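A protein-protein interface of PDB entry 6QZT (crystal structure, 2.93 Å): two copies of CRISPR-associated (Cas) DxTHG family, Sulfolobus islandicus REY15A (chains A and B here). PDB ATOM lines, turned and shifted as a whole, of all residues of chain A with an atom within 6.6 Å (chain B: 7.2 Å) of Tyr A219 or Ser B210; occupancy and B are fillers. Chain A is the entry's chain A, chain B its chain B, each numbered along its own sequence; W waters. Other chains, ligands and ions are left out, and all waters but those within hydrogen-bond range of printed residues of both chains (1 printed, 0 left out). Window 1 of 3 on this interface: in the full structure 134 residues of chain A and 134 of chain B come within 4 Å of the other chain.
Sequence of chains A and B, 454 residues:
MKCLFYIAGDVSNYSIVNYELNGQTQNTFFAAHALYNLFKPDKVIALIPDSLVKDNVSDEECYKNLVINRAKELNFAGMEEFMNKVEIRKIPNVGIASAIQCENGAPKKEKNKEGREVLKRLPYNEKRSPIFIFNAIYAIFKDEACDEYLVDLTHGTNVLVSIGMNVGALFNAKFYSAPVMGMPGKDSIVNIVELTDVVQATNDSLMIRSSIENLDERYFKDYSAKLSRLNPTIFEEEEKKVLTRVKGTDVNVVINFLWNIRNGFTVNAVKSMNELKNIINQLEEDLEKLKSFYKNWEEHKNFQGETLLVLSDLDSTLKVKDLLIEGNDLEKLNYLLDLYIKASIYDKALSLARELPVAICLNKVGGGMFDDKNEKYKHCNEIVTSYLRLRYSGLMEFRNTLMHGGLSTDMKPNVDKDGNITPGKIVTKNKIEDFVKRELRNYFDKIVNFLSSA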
ATOM      1  N   ASN A 203      19.206  -5.496   9.599  1.00  0.00           N
ATOM      2  CA  ASN A 203      19.428  -6.725   8.812  1.00  0.00           C
ATOM      3  C   ASN A 203      18.221  -6.994   7.907  1.00  0.00           C
ATOM      4  O   ASN A 203      18.401  -7.217   6.704  1.00  0.00           O
ATOM      5  CB  ASN A 203      19.697  -7.965   9.697  1.00  0.00           C
ATOM      6  CG  ASN A 203      19.591  -9.320   8.965  1.00  0.00           C
ATOM      7  OD1 ASN A 203      20.355  -9.623   8.037  1.00  0.00           O
ATOM      8  ND2 ASN A 203      18.638 -10.171   9.361  1.00  0.00           N
ATOM      9  N   ASP A 204      16.992  -6.949   8.491  1.00  0.00           N
ATOM     10  CA  ASP A 204      15.727  -7.145   7.785  1.00  0.00           C
ATOM     11  C   ASP A 204      15.675  -6.282   6.527  1.00  0.00           C
ATOM     12  O   ASP A 204      15.384  -6.802   5.455  1.00  0.00           O
ATOM     13  CB  ASP A 204      14.535  -6.831   8.702  1.00  0.00           C
ATOM     14  CG  ASP A 204      14.288  -7.805   9.850  1.00  0.00           C
ATOM     15  OD1 ASP A 204      15.021  -8.828   9.939  1.00  0.00           O
ATOM     16  OD2 ASP A 204      13.359  -7.548  10.660  1.00  0.00           O
ATOM     17  N   LEU A 206      18.323  -4.804   4.907  1.00  0.00           N
ATOM     18  CA  LEU A 206      19.387  -5.180   3.966  1.00  0.00           C
ATOM     19  C   LEU A 206      19.010  -6.414   3.177  1.00  0.00           C
ATOM     20  O   LEU A 206      19.335  -6.505   1.991  1.00  0.00           O
ATOM     21  CB  LEU A 206      20.730  -5.421   4.646  1.00  0.00           C
ATOM     22  CG  LEU A 206      21.316  -4.309   5.496  1.00  0.00           C
ATOM     23  CD1 LEU A 206      22.282  -4.892   6.508  1.00  0.00           C
ATOM     24  CD2 LEU A 206      21.969  -3.226   4.648  1.00  0.00           C
ATOM     25  N   MET A 207      18.320  -7.353   3.837  1.00  0.00           N
ATOM     26  CA  MET A 207      17.826  -8.600   3.250  1.00  0.00           C
ATOM     27  C   MET A 207      16.675  -8.335   2.260  1.00  0.00           C
ATOM     28  O   MET A 207      16.706  -8.830   1.128  1.00  0.00           O
ATOM     29  CB  MET A 207      17.403  -9.579   4.357  1.00  0.00           C
ATOM     30  CG  MET A 207      18.574 -10.210   5.070  1.00  0.00           C
ATOM     31  SD  MET A 207      19.412 -11.462   4.063  1.00  0.00           S
ATOM     32  CE  MET A 207      20.889 -11.652   4.942  1.00  0.00           C
ATOM     33  N   ILE A 208      15.684  -7.518   2.692  1.00  0.00           N
ATOM     34  CA  ILE A 208      14.535  -7.100   1.896  1.00  0.00           C
ATOM     35  C   ILE A 208      15.037  -6.420   0.622  1.00  0.00           C
ATOM     36  O   ILE A 208      14.556  -6.759  -0.453  1.00  0.00           O
ATOM     37  CB  ILE A 208      13.535  -6.243   2.732  1.00  0.00           C
ATOM     38  CG1 ILE A 208      12.705  -7.148   3.676  1.00  0.00           C
ATOM     39  CG2 ILE A 208      12.620  -5.366   1.838  1.00  0.00           C
ATOM     40  CD1 ILE A 208      11.973  -6.435   4.750  1.00  0.00           C
ATOM     41  N   ARG A 209      16.048  -5.543   0.725  1.00  0.00           N
ATOM     42  CA  ARG A 209      16.618  -4.853  -0.444  1.00  0.00           C
ATOM     43  C   ARG A 209      17.223  -5.802  -1.474  1.00  0.00           C
ATOM     44  O   ARG A 209      17.140  -5.513  -2.669  1.00  0.00           O
ATOM     45  CB  ARG A 209      17.633  -3.777  -0.033  1.00  0.00           C
ATOM     46  CG  ARG A 209      16.983  -2.507   0.482  1.00  0.00           C
ATOM     47  CD  ARG A 209      17.912  -1.743   1.395  1.00  0.00           C
ATOM     48  NE  ARG A 209      17.201  -0.675   2.102  1.00  0.00           N
ATOM     49  CZ  ARG A 209      17.758   0.468   2.490  1.00  0.00           C
ATOM     50  NH1 ARG A 209      19.040   0.708   2.241  1.00  0.00           N
ATOM     51  NH2 ARG A 209      17.031   1.390   3.112  1.00  0.00           N
ATOM     52  N   SER A 210      17.799  -6.936  -1.024  1.00  0.00           N
ATOM     53  CA  SER A 210      18.367  -7.940  -1.919  1.00  0.00           C
ATOM     54  C   SER A 210      17.280  -8.823  -2.543  1.00  0.00           C
ATOM     55  O   SER A 210      17.517  -9.348  -3.623  1.00  0.00           O
ATOM     56  CB  SER A 210      19.422  -8.782  -1.209  1.00  0.00           C
ATOM     57  OG  SER A 210      18.834  -9.721  -0.325  1.00  0.00           O
ATOM     58  N   SER A 211      16.092  -8.985  -1.878  1.00  0.00           N
ATOM     59  CA  SER A 211      14.957  -9.772  -2.391  1.00  0.00           C
ATOM     60  C   SER A 211      14.534  -9.222  -3.706  1.00  0.00           C
ATOM     61  O   SER A 211      14.172  -9.962  -4.612  1.00  0.00           O
ATOM     62  CB  SER A 211      13.745  -9.659  -1.483  1.00  0.00           C
ATOM     63  OG  SER A 211      14.087  -9.968  -0.152  1.00  0.00           O
ATOM     64  N   ILE A 212      14.531  -7.907  -3.786  1.00  0.00           N
ATOM     65  CA  ILE A 212      14.162  -7.163  -4.961  1.00  0.00           C
ATOM     66  C   ILE A 212      15.331  -7.256  -5.938  1.00  0.00           C
ATOM     67  O   ILE A 212      15.145  -7.718  -7.070  1.00  0.00           O
ATOM     68  CB  ILE A 212      13.808  -5.707  -4.516  1.00  0.00           C
ATOM     69  CG1 ILE A 212      12.535  -5.704  -3.613  1.00  0.00           C
ATOM     70  CG2 ILE A 212      13.655  -4.749  -5.714  1.00  0.00           C
ATOM     71  CD1 ILE A 212      12.588  -4.773  -2.392  1.00  0.00           C
ATOM     72  N   ASN A 214      17.906  -9.284  -6.356  1.00  0.00           N
ATOM     73  CA  ASN A 214      18.144 -10.629  -6.880  1.00  0.00           C
ATOM     74  C   ASN A 214      16.878 -11.448  -7.172  1.00  0.00           C
ATOM     75  O   ASN A 214      16.991 -12.662  -7.406  1.00  0.00           O
ATOM     76  CB  ASN A 214      19.076 -11.407  -5.941  1.00  0.00           C
ATOM     77  CG  ASN A 214      20.433 -10.773  -5.749  1.00  0.00           C
ATOM     78  OD1 ASN A 214      21.191 -10.545  -6.707  1.00  0.00           O
ATOM     79  ND2 ASN A 214      20.769 -10.477  -4.500  1.00  0.00           N
ATOM     80  N   ASP A 216      14.531 -12.668  -5.344  1.00  0.00           N
ATOM     81  CA  ASP A 216      14.416 -13.838  -4.506  1.00  0.00           C
ATOM     82  C   ASP A 216      13.627 -13.500  -3.236  1.00  0.00           C
ATOM     83  O   ASP A 216      14.114 -12.741  -2.403  1.00  0.00           O
ATOM     84  CB  ASP A 216      15.825 -14.363  -4.192  1.00  0.00           C
ATOM     85  CG  ASP A 216      15.902 -15.785  -3.666  1.00  0.00           C
ATOM     86  OD1 ASP A 216      14.900 -16.266  -3.083  1.00  0.00           O
ATOM     87  OD2 ASP A 216      16.966 -16.410  -3.816  1.00  0.00           O
ATOM     88  N   GLU A 217      12.415 -14.080  -3.088  1.00  0.00           N
ATOM     89  CA  GLU A 217      11.502 -13.885  -1.946  1.00  0.00           C
ATOM     90  C   GLU A 217      11.932 -14.587  -0.665  1.00  0.00           C
ATOM     91  O   GLU A 217      11.348 -14.350   0.407  1.00  0.00           O
ATOM     92  CB  GLU A 217      10.088 -14.331  -2.298  1.00  0.00           C
ATOM     93  CG  GLU A 217      10.046 -15.620  -3.090  1.00  0.00           C
ATOM     94  CD  GLU A 217      10.204 -16.925  -2.350  1.00  0.00           C
ATOM     95  OE1 GLU A 217       9.868 -16.998  -1.146  1.00  0.00           O
ATOM     96  OE2 GLU A 217      10.651 -17.893  -2.999  1.00  0.00           O
ATOM     97  N   ARG A 218      12.904 -15.491  -0.772  1.00  0.00           N
ATOM     98  CA  ARG A 218      13.404 -16.191   0.402  1.00  0.00           C
ATOM     99  C   ARG A 218      14.156 -15.217   1.337  1.00  0.00           C
ATOM    100  O   ARG A 218      14.314 -15.508   2.528  1.00  0.00           O
ATOM    101  CB  ARG A 218      14.286 -17.373  -0.011  1.00  0.00           C
ATOM    102  CG  ARG A 218      13.599 -18.370  -0.946  1.00  0.00           C
ATOM    103  CD  ARG A 218      14.537 -19.458  -1.440  1.00  0.00           C
ATOM    104  NE  ARG A 218      15.668 -18.925  -2.206  1.00  0.00           N
ATOM    105  CZ  ARG A 218      16.681 -19.662  -2.653  1.00  0.00           C
ATOM    106  NH1 ARG A 218      16.705 -20.975  -2.440  1.00  0.00           N
ATOM    107  NH2 ARG A 218      17.670 -19.097  -3.336  1.00  0.00           N
ATOM    108  N   TYR A 219      14.568 -14.046   0.800  1.00  0.00           N
ATOM    109  CA  TYR A 219      15.278 -12.973   1.505  1.00  0.00           C
ATOM    110  C   TYR A 219      14.327 -11.909   2.073  1.00  0.00           C
ATOM    111  O   TYR A 219      14.721 -11.104   2.921  1.00  0.00           O
ATOM    112  CB  TYR A 219      16.376 -12.364   0.595  1.00  0.00           C
ATOM    113  CG  TYR A 219      17.457 -13.377   0.288  1.00  0.00           C
ATOM    114  CD1 TYR A 219      17.319 -14.274  -0.770  1.00  0.00           C
ATOM    115  CD2 TYR A 219      18.540 -13.545   1.144  1.00  0.00           C
ATOM    116  CE1 TYR A 219      18.238 -15.308  -0.974  1.00  0.00           C
ATOM    117  CE2 TYR A 219      19.478 -14.562   0.937  1.00  0.00           C
ATOM    118  CZ  TYR A 219      19.332 -15.432  -0.133  1.00  0.00           C
ATOM    119  OH  TYR A 219      20.267 -16.419  -0.352  1.00  0.00           O
ATOM    120  N   PHE A 220      13.072 -11.909   1.612  1.00  0.00           N
ATOM    121  CA  PHE A 220      12.081 -10.956   2.097  1.00  0.00           C
ATOM    122  C   PHE A 220      11.574 -11.377   3.469  1.00  0.00           C
ATOM    123  O   PHE A 220      11.068 -12.496   3.616  1.00  0.00           O
ATOM    124  CB  PHE A 220      10.927 -10.806   1.105  1.00  0.00           C
ATOM    125  CG  PHE A 220      10.243  -9.471   1.201  1.00  0.00           C
ATOM    126  CD1 PHE A 220       9.297  -9.226   2.187  1.00  0.00           C
ATOM    127  CD2 PHE A 220      10.553  -8.450   0.313  1.00  0.00           C
ATOM    128  CE1 PHE A 220       8.669  -7.987   2.280  1.00  0.00           C
ATOM    129  CE2 PHE A 220       9.911  -7.213   0.395  1.00  0.00           C
ATOM    130  CZ  PHE A 220       8.975  -6.987   1.383  1.00  0.00           C
ATOM    131  N   LYS A 221      11.744 -10.481   4.476  1.00  0.00           N
ATOM    132  CA  LYS A 221      11.303 -10.700   5.858  1.00  0.00           C
ATOM    133  C   LYS A 221       9.869 -10.226   5.978  1.00  0.00           C
ATOM    134  O   LYS A 221       9.591  -9.056   5.707  1.00  0.00           O
ATOM    135  CB  LYS A 221      12.223  -9.993   6.883  1.00  0.00           C
ATOM    136  CG  LYS A 221      13.732 -10.231   6.681  1.00  0.00           C
ATOM    137  CD  LYS A 221      14.184 -11.678   6.949  1.00  0.00           C
ATOM    138  CE  LYS A 221      15.661 -11.884   6.723  1.00  0.00           C
ATOM    139  NZ  LYS A 221      16.007 -13.332   6.614  1.00  0.00           N
ATOM    140  N   ASP B 204      28.645  -8.860   5.322  1.00  0.00           N
ATOM    141  CA  ASP B 204      29.312  -9.865   4.497  1.00  0.00           C
ATOM    142  C   ASP B 204      29.081 -11.251   5.072  1.00  0.00           C
ATOM    143  O   ASP B 204      28.675 -12.136   4.335  1.00  0.00           O
ATOM    144  CB  ASP B 204      30.823  -9.578   4.375  1.00  0.00           C
ATOM    145  CG  ASP B 204      31.214  -8.358   3.550  1.00  0.00           C
ATOM    146  OD1 ASP B 204      30.297  -7.704   2.968  1.00  0.00           O
ATOM    147  OD2 ASP B 204      32.439  -8.052   3.480  1.00  0.00           O
ATOM    148  N   SER B 205      29.253 -11.411   6.401  1.00  0.00           N
ATOM    149  CA  SER B 205      29.063 -12.680   7.105  1.00  0.00           C
ATOM    150  C   SER B 205      27.630 -13.138   7.110  1.00  0.00           C
ATOM    151  O   SER B 205      27.401 -14.316   6.874  1.00  0.00           O
ATOM    152  CB  SER B 205      29.642 -12.638   8.515  1.00  0.00           C
ATOM    153  OG  SER B 205      31.054 -12.503   8.448  1.00  0.00           O
ATOM    154  N   LEU B 206      26.663 -12.224   7.316  1.00  0.00           N
ATOM    155  CA  LEU B 206      25.233 -12.574   7.318  1.00  0.00           C
ATOM    156  C   LEU B 206      24.794 -13.029   5.956  1.00  0.00           C
ATOM    157  O   LEU B 206      23.968 -13.937   5.857  1.00  0.00           O
ATOM    158  CB  LEU B 206      24.336 -11.402   7.756  1.00  0.00           C
ATOM    159  CG  LEU B 206      24.599 -10.764   9.103  1.00  0.00           C
ATOM    160  CD1 LEU B 206      24.057  -9.354   9.126  1.00  0.00           C
ATOM    161  CD2 LEU B 206      24.025 -11.585  10.211  1.00  0.00           C
ATOM    162  N   MET B 207      25.343 -12.392   4.911  1.00  0.00           N
ATOM    163  CA  MET B 207      25.073 -12.686   3.504  1.00  0.00           C
ATOM    164  C   MET B 207      25.697 -14.036   3.081  1.00  0.00           C
ATOM    165  O   MET B 207      25.023 -14.868   2.470  1.00  0.00           O
ATOM    166  CB  MET B 207      25.567 -11.536   2.620  1.00  0.00           C
ATOM    167  CG  MET B 207      24.686 -10.309   2.696  1.00  0.00           C
ATOM    168  SD  MET B 207      23.096 -10.540   1.883  1.00  0.00           S
ATOM    169  CE  MET B 207      22.216  -9.144   2.491  1.00  0.00           C
ATOM    170  N   ILE B 208      26.978 -14.249   3.436  1.00  0.00           N
ATOM    171  CA  ILE B 208      27.724 -15.473   3.180  1.00  0.00           C
ATOM    172  C   ILE B 208      26.962 -16.634   3.802  1.00  0.00           C
ATOM    173  O   ILE B 208      26.764 -17.632   3.126  1.00  0.00           O
ATOM    174  CB  ILE B 208      29.212 -15.350   3.644  1.00  0.00           C
ATOM    175  CG1 ILE B 208      30.026 -14.522   2.623  1.00  0.00           C
ATOM    176  CG2 ILE B 208      29.867 -16.715   3.894  1.00  0.00           C
ATOM    177  CD1 ILE B 208      31.351 -14.063   3.099  1.00  0.00           C
ATOM    178  N   ARG B 209      26.452 -16.478   5.038  1.00  0.00           N
ATOM    179  CA  ARG B 209      25.690 -17.534   5.725  1.00  0.00           C
ATOM    180  C   ARG B 209      24.389 -17.862   4.992  1.00  0.00           C
ATOM    181  O   ARG B 209      23.963 -19.016   4.980  1.00  0.00           O
ATOM    182  CB  ARG B 209      25.403 -17.152   7.185  1.00  0.00           C
ATOM    183  CG  ARG B 209      26.601 -17.316   8.100  1.00  0.00           C
ATOM    184  CD  ARG B 209      26.482 -16.434   9.325  1.00  0.00           C
ATOM    185  NE  ARG B 209      27.735 -16.404  10.081  1.00  0.00           N
ATOM    186  CZ  ARG B 209      27.818 -16.162  11.385  1.00  0.00           C
ATOM    187  NH1 ARG B 209      26.721 -15.898  12.092  1.00  0.00           N
ATOM    188  NH2 ARG B 209      28.999 -16.158  11.990  1.00  0.00           N
ATOM    189  N   SER B 210      23.784 -16.832   4.367  1.00  0.00           N
ATOM    190  CA  SER B 210      22.537 -16.979   3.628  1.00  0.00           C
ATOM    191  C   SER B 210      22.803 -17.654   2.310  1.00  0.00           C
ATOM    192  O   SER B 210      22.009 -18.493   1.899  1.00  0.00           O
ATOM    193  CB  SER B 210      21.865 -15.626   3.407  1.00  0.00           C
ATOM    194  OG  SER B 210      22.275 -15.031   2.187  1.00  0.00           O
ATOM    195  N   SER B 211      23.920 -17.288   1.641  1.00  0.00           N
ATOM    196  CA  SER B 211      24.314 -17.868   0.356  1.00  0.00           C
ATOM    197  C   SER B 211      24.392 -19.386   0.481  1.00  0.00           C
ATOM    198  O   SER B 211      24.034 -20.094  -0.452  1.00  0.00           O
ATOM    199  CB  SER B 211      25.651 -17.300  -0.104  1.00  0.00           C
ATOM    200  OG  SER B 211      26.735 -18.168   0.182  1.00  0.00           O
ATOM    201  N   ILE B 212      24.815 -19.870   1.653  1.00  0.00           N
ATOM    202  CA  ILE B 212      24.952 -21.288   1.936  1.00  0.00           C
ATOM    203  C   ILE B 212      23.578 -21.881   2.238  1.00  0.00           C
ATOM    204  O   ILE B 212      23.239 -22.961   1.759  1.00  0.00           O
ATOM    205  CB  ILE B 212      26.027 -21.516   3.036  1.00  0.00           C
ATOM    206  CG1 ILE B 212      27.421 -21.134   2.504  1.00  0.00           C
ATOM    207  CG2 ILE B 212      26.025 -22.962   3.540  1.00  0.00           C
ATOM    208  CD1 ILE B 212      28.344 -20.648   3.516  1.00  0.00           C
ATOM    209  N   GLU B 213      22.780 -21.156   2.999  1.00  0.00           N
ATOM    210  CA  GLU B 213      21.431 -21.560   3.404  1.00  0.00           C
ATOM    211  C   GLU B 213      20.523 -21.736   2.184  1.00  0.00           C
ATOM    212  O   GLU B 213      19.861 -22.769   2.074  1.00  0.00           O
ATOM    213  CB  GLU B 213      20.855 -20.516   4.405  1.00  0.00           C
ATOM    214  CG  GLU B 213      19.611 -20.943   5.186  1.00  0.00           C
ATOM    215  CD  GLU B 213      18.584 -19.842   5.424  1.00  0.00           C
ATOM    216  OE1 GLU B 213      18.974 -18.742   5.889  1.00  0.00           O
ATOM    217  OE2 GLU B 213      17.384 -20.085   5.149  1.00  0.00           O
ATOM    218  N   ASN B 214      20.554 -20.762   1.251  1.00  0.00           N
ATOM    219  CA  ASN B 214      19.716 -20.708   0.058  1.00  0.00           C
ATOM    220  C   ASN B 214      20.414 -21.167  -1.232  1.00  0.00           C
ATOM    221  O   ASN B 214      19.836 -20.993  -2.307  1.00  0.00           O
ATOM    222  CB  ASN B 214      19.125 -19.309  -0.107  1.00  0.00           C
ATOM    223  CG  ASN B 214      18.240 -18.879   1.030  1.00  0.00           C
ATOM    224  OD1 ASN B 214      17.248 -19.531   1.370  1.00  0.00           O
ATOM    225  ND2 ASN B 214      18.578 -17.769   1.651  1.00  0.00           N
ATOM    226  N   LEU B 215      21.622 -21.788  -1.132  1.00  0.00           N
ATOM    227  CA  LEU B 215      22.375 -22.356  -2.278  1.00  0.00           C
ATOM    228  C   LEU B 215      22.525 -21.334  -3.426  1.00  0.00           C
ATOM    229  O   LEU B 215      22.279 -21.667  -4.589  1.00  0.00           O
ATOM    230  CB  LEU B 215      21.633 -23.610  -2.801  1.00  0.00           C
ATOM    231  CG  LEU B 215      21.482 -24.862  -1.945  1.00  0.00           C
ATOM    232  CD1 LEU B 215      20.611 -25.923  -2.565  1.00  0.00           C
ATOM    233  CD2 LEU B 215      22.818 -25.430  -1.638  1.00  0.00           C
ATOM    234  N   ASP B 216      22.894 -20.090  -3.083  1.00  0.00           N
ATOM    235  CA  ASP B 216      22.942 -18.983  -4.024  1.00  0.00           C
ATOM    236  C   ASP B 216      24.227 -18.181  -3.908  1.00  0.00           C
ATOM    237  O   ASP B 216      24.289 -17.239  -3.113  1.00  0.00           O
ATOM    238  CB  ASP B 216      21.721 -18.076  -3.759  1.00  0.00           C
ATOM    239  CG  ASP B 216      21.395 -17.080  -4.851  1.00  0.00           C
ATOM    240  OD1 ASP B 216      22.326 -16.638  -5.549  1.00  0.00           O
ATOM    241  OD2 ASP B 216      20.205 -16.734  -5.001  1.00  0.00           O
ATOM    242  N   GLU B 217      25.218 -18.483  -4.761  1.00  0.00           N
ATOM    243  CA  GLU B 217      26.498 -17.763  -4.798  1.00  0.00           C
ATOM    244  C   GLU B 217      26.380 -16.219  -4.978  1.00  0.00           C
ATOM    245  O   GLU B 217      27.379 -15.524  -4.757  1.00  0.00           O
ATOM    246  CB  GLU B 217      27.416 -18.359  -5.875  1.00  0.00           C
ATOM    247  CG  GLU B 217      27.279 -17.754  -7.267  1.00  0.00           C
ATOM    248  CD  GLU B 217      25.939 -17.821  -7.976  1.00  0.00           C
ATOM    249  OE1 GLU B 217      25.140 -18.729  -7.652  1.00  0.00           O
ATOM    250  OE2 GLU B 217      25.702 -16.974  -8.871  1.00  0.00           O
ATOM    251  N   ARG B 218      25.186 -15.684  -5.390  1.00  0.00           N
ATOM    252  CA  ARG B 218      25.018 -14.234  -5.566  1.00  0.00           C
ATOM    253  C   ARG B 218      25.135 -13.501  -4.238  1.00  0.00           C
ATOM    254  O   ARG B 218      25.448 -12.308  -4.243  1.00  0.00           O
ATOM    255  CB  ARG B 218      23.708 -13.861  -6.279  1.00  0.00           C
ATOM    256  CG  ARG B 218      23.537 -14.490  -7.656  1.00  0.00           C
ATOM    257  CD  ARG B 218      22.178 -14.224  -8.271  1.00  0.00           C
ATOM    258  NE  ARG B 218      21.079 -14.693  -7.426  1.00  0.00           N
ATOM    259  CZ  ARG B 218      19.798 -14.476  -7.696  1.00  0.00           C
ATOM    260  NH1 ARG B 218      19.447 -13.804  -8.788  1.00  0.00           N
ATOM    261  NH2 ARG B 218      18.853 -14.924  -6.873  1.00  0.00           N
ATOM    262  N   TYR B 219      24.927 -14.231  -3.110  1.00  0.00           N
ATOM    263  CA  TYR B 219      25.001 -13.721  -1.735  1.00  0.00           C
ATOM    264  C   TYR B 219      26.392 -13.895  -1.122  1.00  0.00           C
ATOM    265  O   TYR B 219      26.717 -13.226  -0.136  1.00  0.00           O
ATOM    266  CB  TYR B 219      23.879 -14.331  -0.859  1.00  0.00           C
ATOM    267  CG  TYR B 219      22.516 -13.883  -1.333  1.00  0.00           C
ATOM    268  CD1 TYR B 219      21.859 -14.554  -2.362  1.00  0.00           C
ATOM    269  CD2 TYR B 219      21.953 -12.698  -0.868  1.00  0.00           C
ATOM    270  CE1 TYR B 219      20.666 -14.066  -2.897  1.00  0.00           C
ATOM    271  CE2 TYR B 219      20.751 -12.212  -1.382  1.00  0.00           C
ATOM    272  CZ  TYR B 219      20.104 -12.902  -2.390  1.00  0.00           C
ATOM    273  OH  TYR B 219      18.904 -12.418  -2.862  1.00  0.00           O
ATOM    274  N   PHE B 220      27.232 -14.749  -1.733  1.00  0.00           N
ATOM    275  CA  PHE B 220      28.594 -14.957  -1.253  1.00  0.00           C
ATOM    276  C   PHE B 220      29.468 -13.784  -1.631  1.00  0.00           C
ATOM    277  O   PHE B 220      29.580 -13.475  -2.819  1.00  0.00           O
ATOM    278  CB  PHE B 220      29.189 -16.261  -1.789  1.00  0.00           C
ATOM    279  CG  PHE B 220      30.245 -16.832  -0.886  1.00  0.00           C
ATOM    280  CD1 PHE B 220      31.548 -16.345  -0.915  1.00  0.00           C
ATOM    281  CD2 PHE B 220      29.934 -17.835   0.033  1.00  0.00           C
ATOM    282  CE1 PHE B 220      32.523 -16.869  -0.055  1.00  0.00           C
ATOM    283  CE2 PHE B 220      30.911 -18.363   0.885  1.00  0.00           C
ATOM    284  CZ  PHE B 220      32.196 -17.880   0.835  1.00  0.00           C
HETATM  285  O   HOH W   1      15.292 -17.808   4.509  1.00  0.00           O
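The backbone carbonyl oxygen (O) of Ser A210 lies within hydrogen-bond range of the side-chain hydroxyl (OH) of Tyr B219 (3.5 Å).
The guanidinium group (NH2) of Arg B218 is in hydrogen-bond range of the backbone carbonyl oxygen (O) of Asn A214 (3.0 Å).
The side-chain amide nitrogen (ND2) of Asn A214 is in hydrogen-bond range of the side-chain hydroxyl (OH) of Tyr B219 (3.2 Å).
The guanidinium group (NH2) of Arg B218 is in salt-bridge range of the side-chain carboxylate (OD2) of Asp A216 (3.9 Å).
NH2 of Arg A218 sits at hydrogen-bond distance from O of Asn B214.
NH2 of Arg A218 is in salt-bridge range of OD2 of Asp B216 (3.8 Å).
The side-chain amide nitrogen (ND2) of Asn B214 lies within hydrogen-bond range of the side-chain hydroxyl (OH) of Tyr A219 (2.9 Å).
OD2 of Asp A216 lies close to OD2 of Asp B216 (3.5 Å).
The side-chain hydroxyl of Ser A210 is in hydrogen-bond range of the backbone carbonyl oxygen of Met A207.
The side-chain hydroxyl (OG) of Ser A211 sits at hydrogen-bond distance from the backbone carbonyl oxygen (O) of Met A207 (3.1 Å).
The backbone carbonyl oxygen of Ser A211 is in hydrogen-bond range of the backbone NH of Asp A216.
The side-chain hydroxyl (OG) of Ser A211 lies close to the backbone carbonyl oxygen (O) of Tyr A219 (3.3 Å).
O of Met B207 lies within hydrogen-bond range of OG of Ser B210, 2.8 Å away.
The side-chain carboxylate (OD2) of Asp B216 is in salt-bridge range of the guanidinium group (NH2) of Arg B218 (2.9 Å).
Among the printed residues, merely in contact across the chains: Asn A203 with Leu B206 (3.9 Å), Leu A206 with Met B207 (3.9 Å), Met A207 with Leu B206 (3.9 Å), Met A207 with Met B207 (3.7 Å), Asp A216 with Tyr B219 (3.9 Å), Tyr A219 with Ser B210 (3.1 Å) and Tyr A219 with Tyr B219 (3.2 Å).
Of the printed residues of chain B, Tyr A219 touches Ser B210, Asn B214 and Tyr B219.
Of the printed residues of chain A, Met B207 touches Leu A206 (3.9 Å) and Met A207 (3.7 Å).
Of chain A, only Tyr A219 (3.1 Å) comes within 4 Å of Ser B210.
Of the printed residues of chain A, Asn B214 touches Arg A218 (3.1 Å) and Tyr A219 (2.9 Å).
Printed residues of chain A within 4 Å of Asp B216: Asp A216 (3.5 Å) and Arg A218 (3.8 Å).
Printed residues of chain A within 4 Å of Arg B218: Asn A214 (3.0 Å) and Asp A216 (3.9 Å).
The nearest residue of chain B that does not touch Tyr A219 is Asp B216 (4.1 Å).
The nearest residue of chain A that does not touch Ser B210 is Met A207 (4.4 Å).
The nearest printed residue of chain A that does not touch Tyr B219 is Ser A211 (4.5 Å).
Of the 16 printed residues of chain A, 8 touch a printed residue of chain B.
Of the 17 printed residues of chain B, 7 touch a printed residue of chain A.
Hydrophobic or aromatic side chains of chain B within 4 Å of the printed part of chain A: Leu B206, Met B207 and Tyr B219.
Among the printed residues, 15 pairs touch across the chains.
Leu A206 touches Met B207, and with the chains exchanged Met A207 touches Leu B206.
Ser A210 touches Tyr B219, and with the chains exchanged Tyr A219 touches Ser B210.
Asn A214 touches Tyr B219, and with the chains exchanged Tyr A219 touches Asn B214.
Asp A216 touches Tyr B219, but with the chains exchanged Tyr A219 does not touch Asp B216 (4.1 Å).
Of the 15 pairs that touch across the chains among the printed residues, 13 have their exchanged pair printed and touching as well.
Water W1 bridges OE2 of Glu B213 and O of Arg A218.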
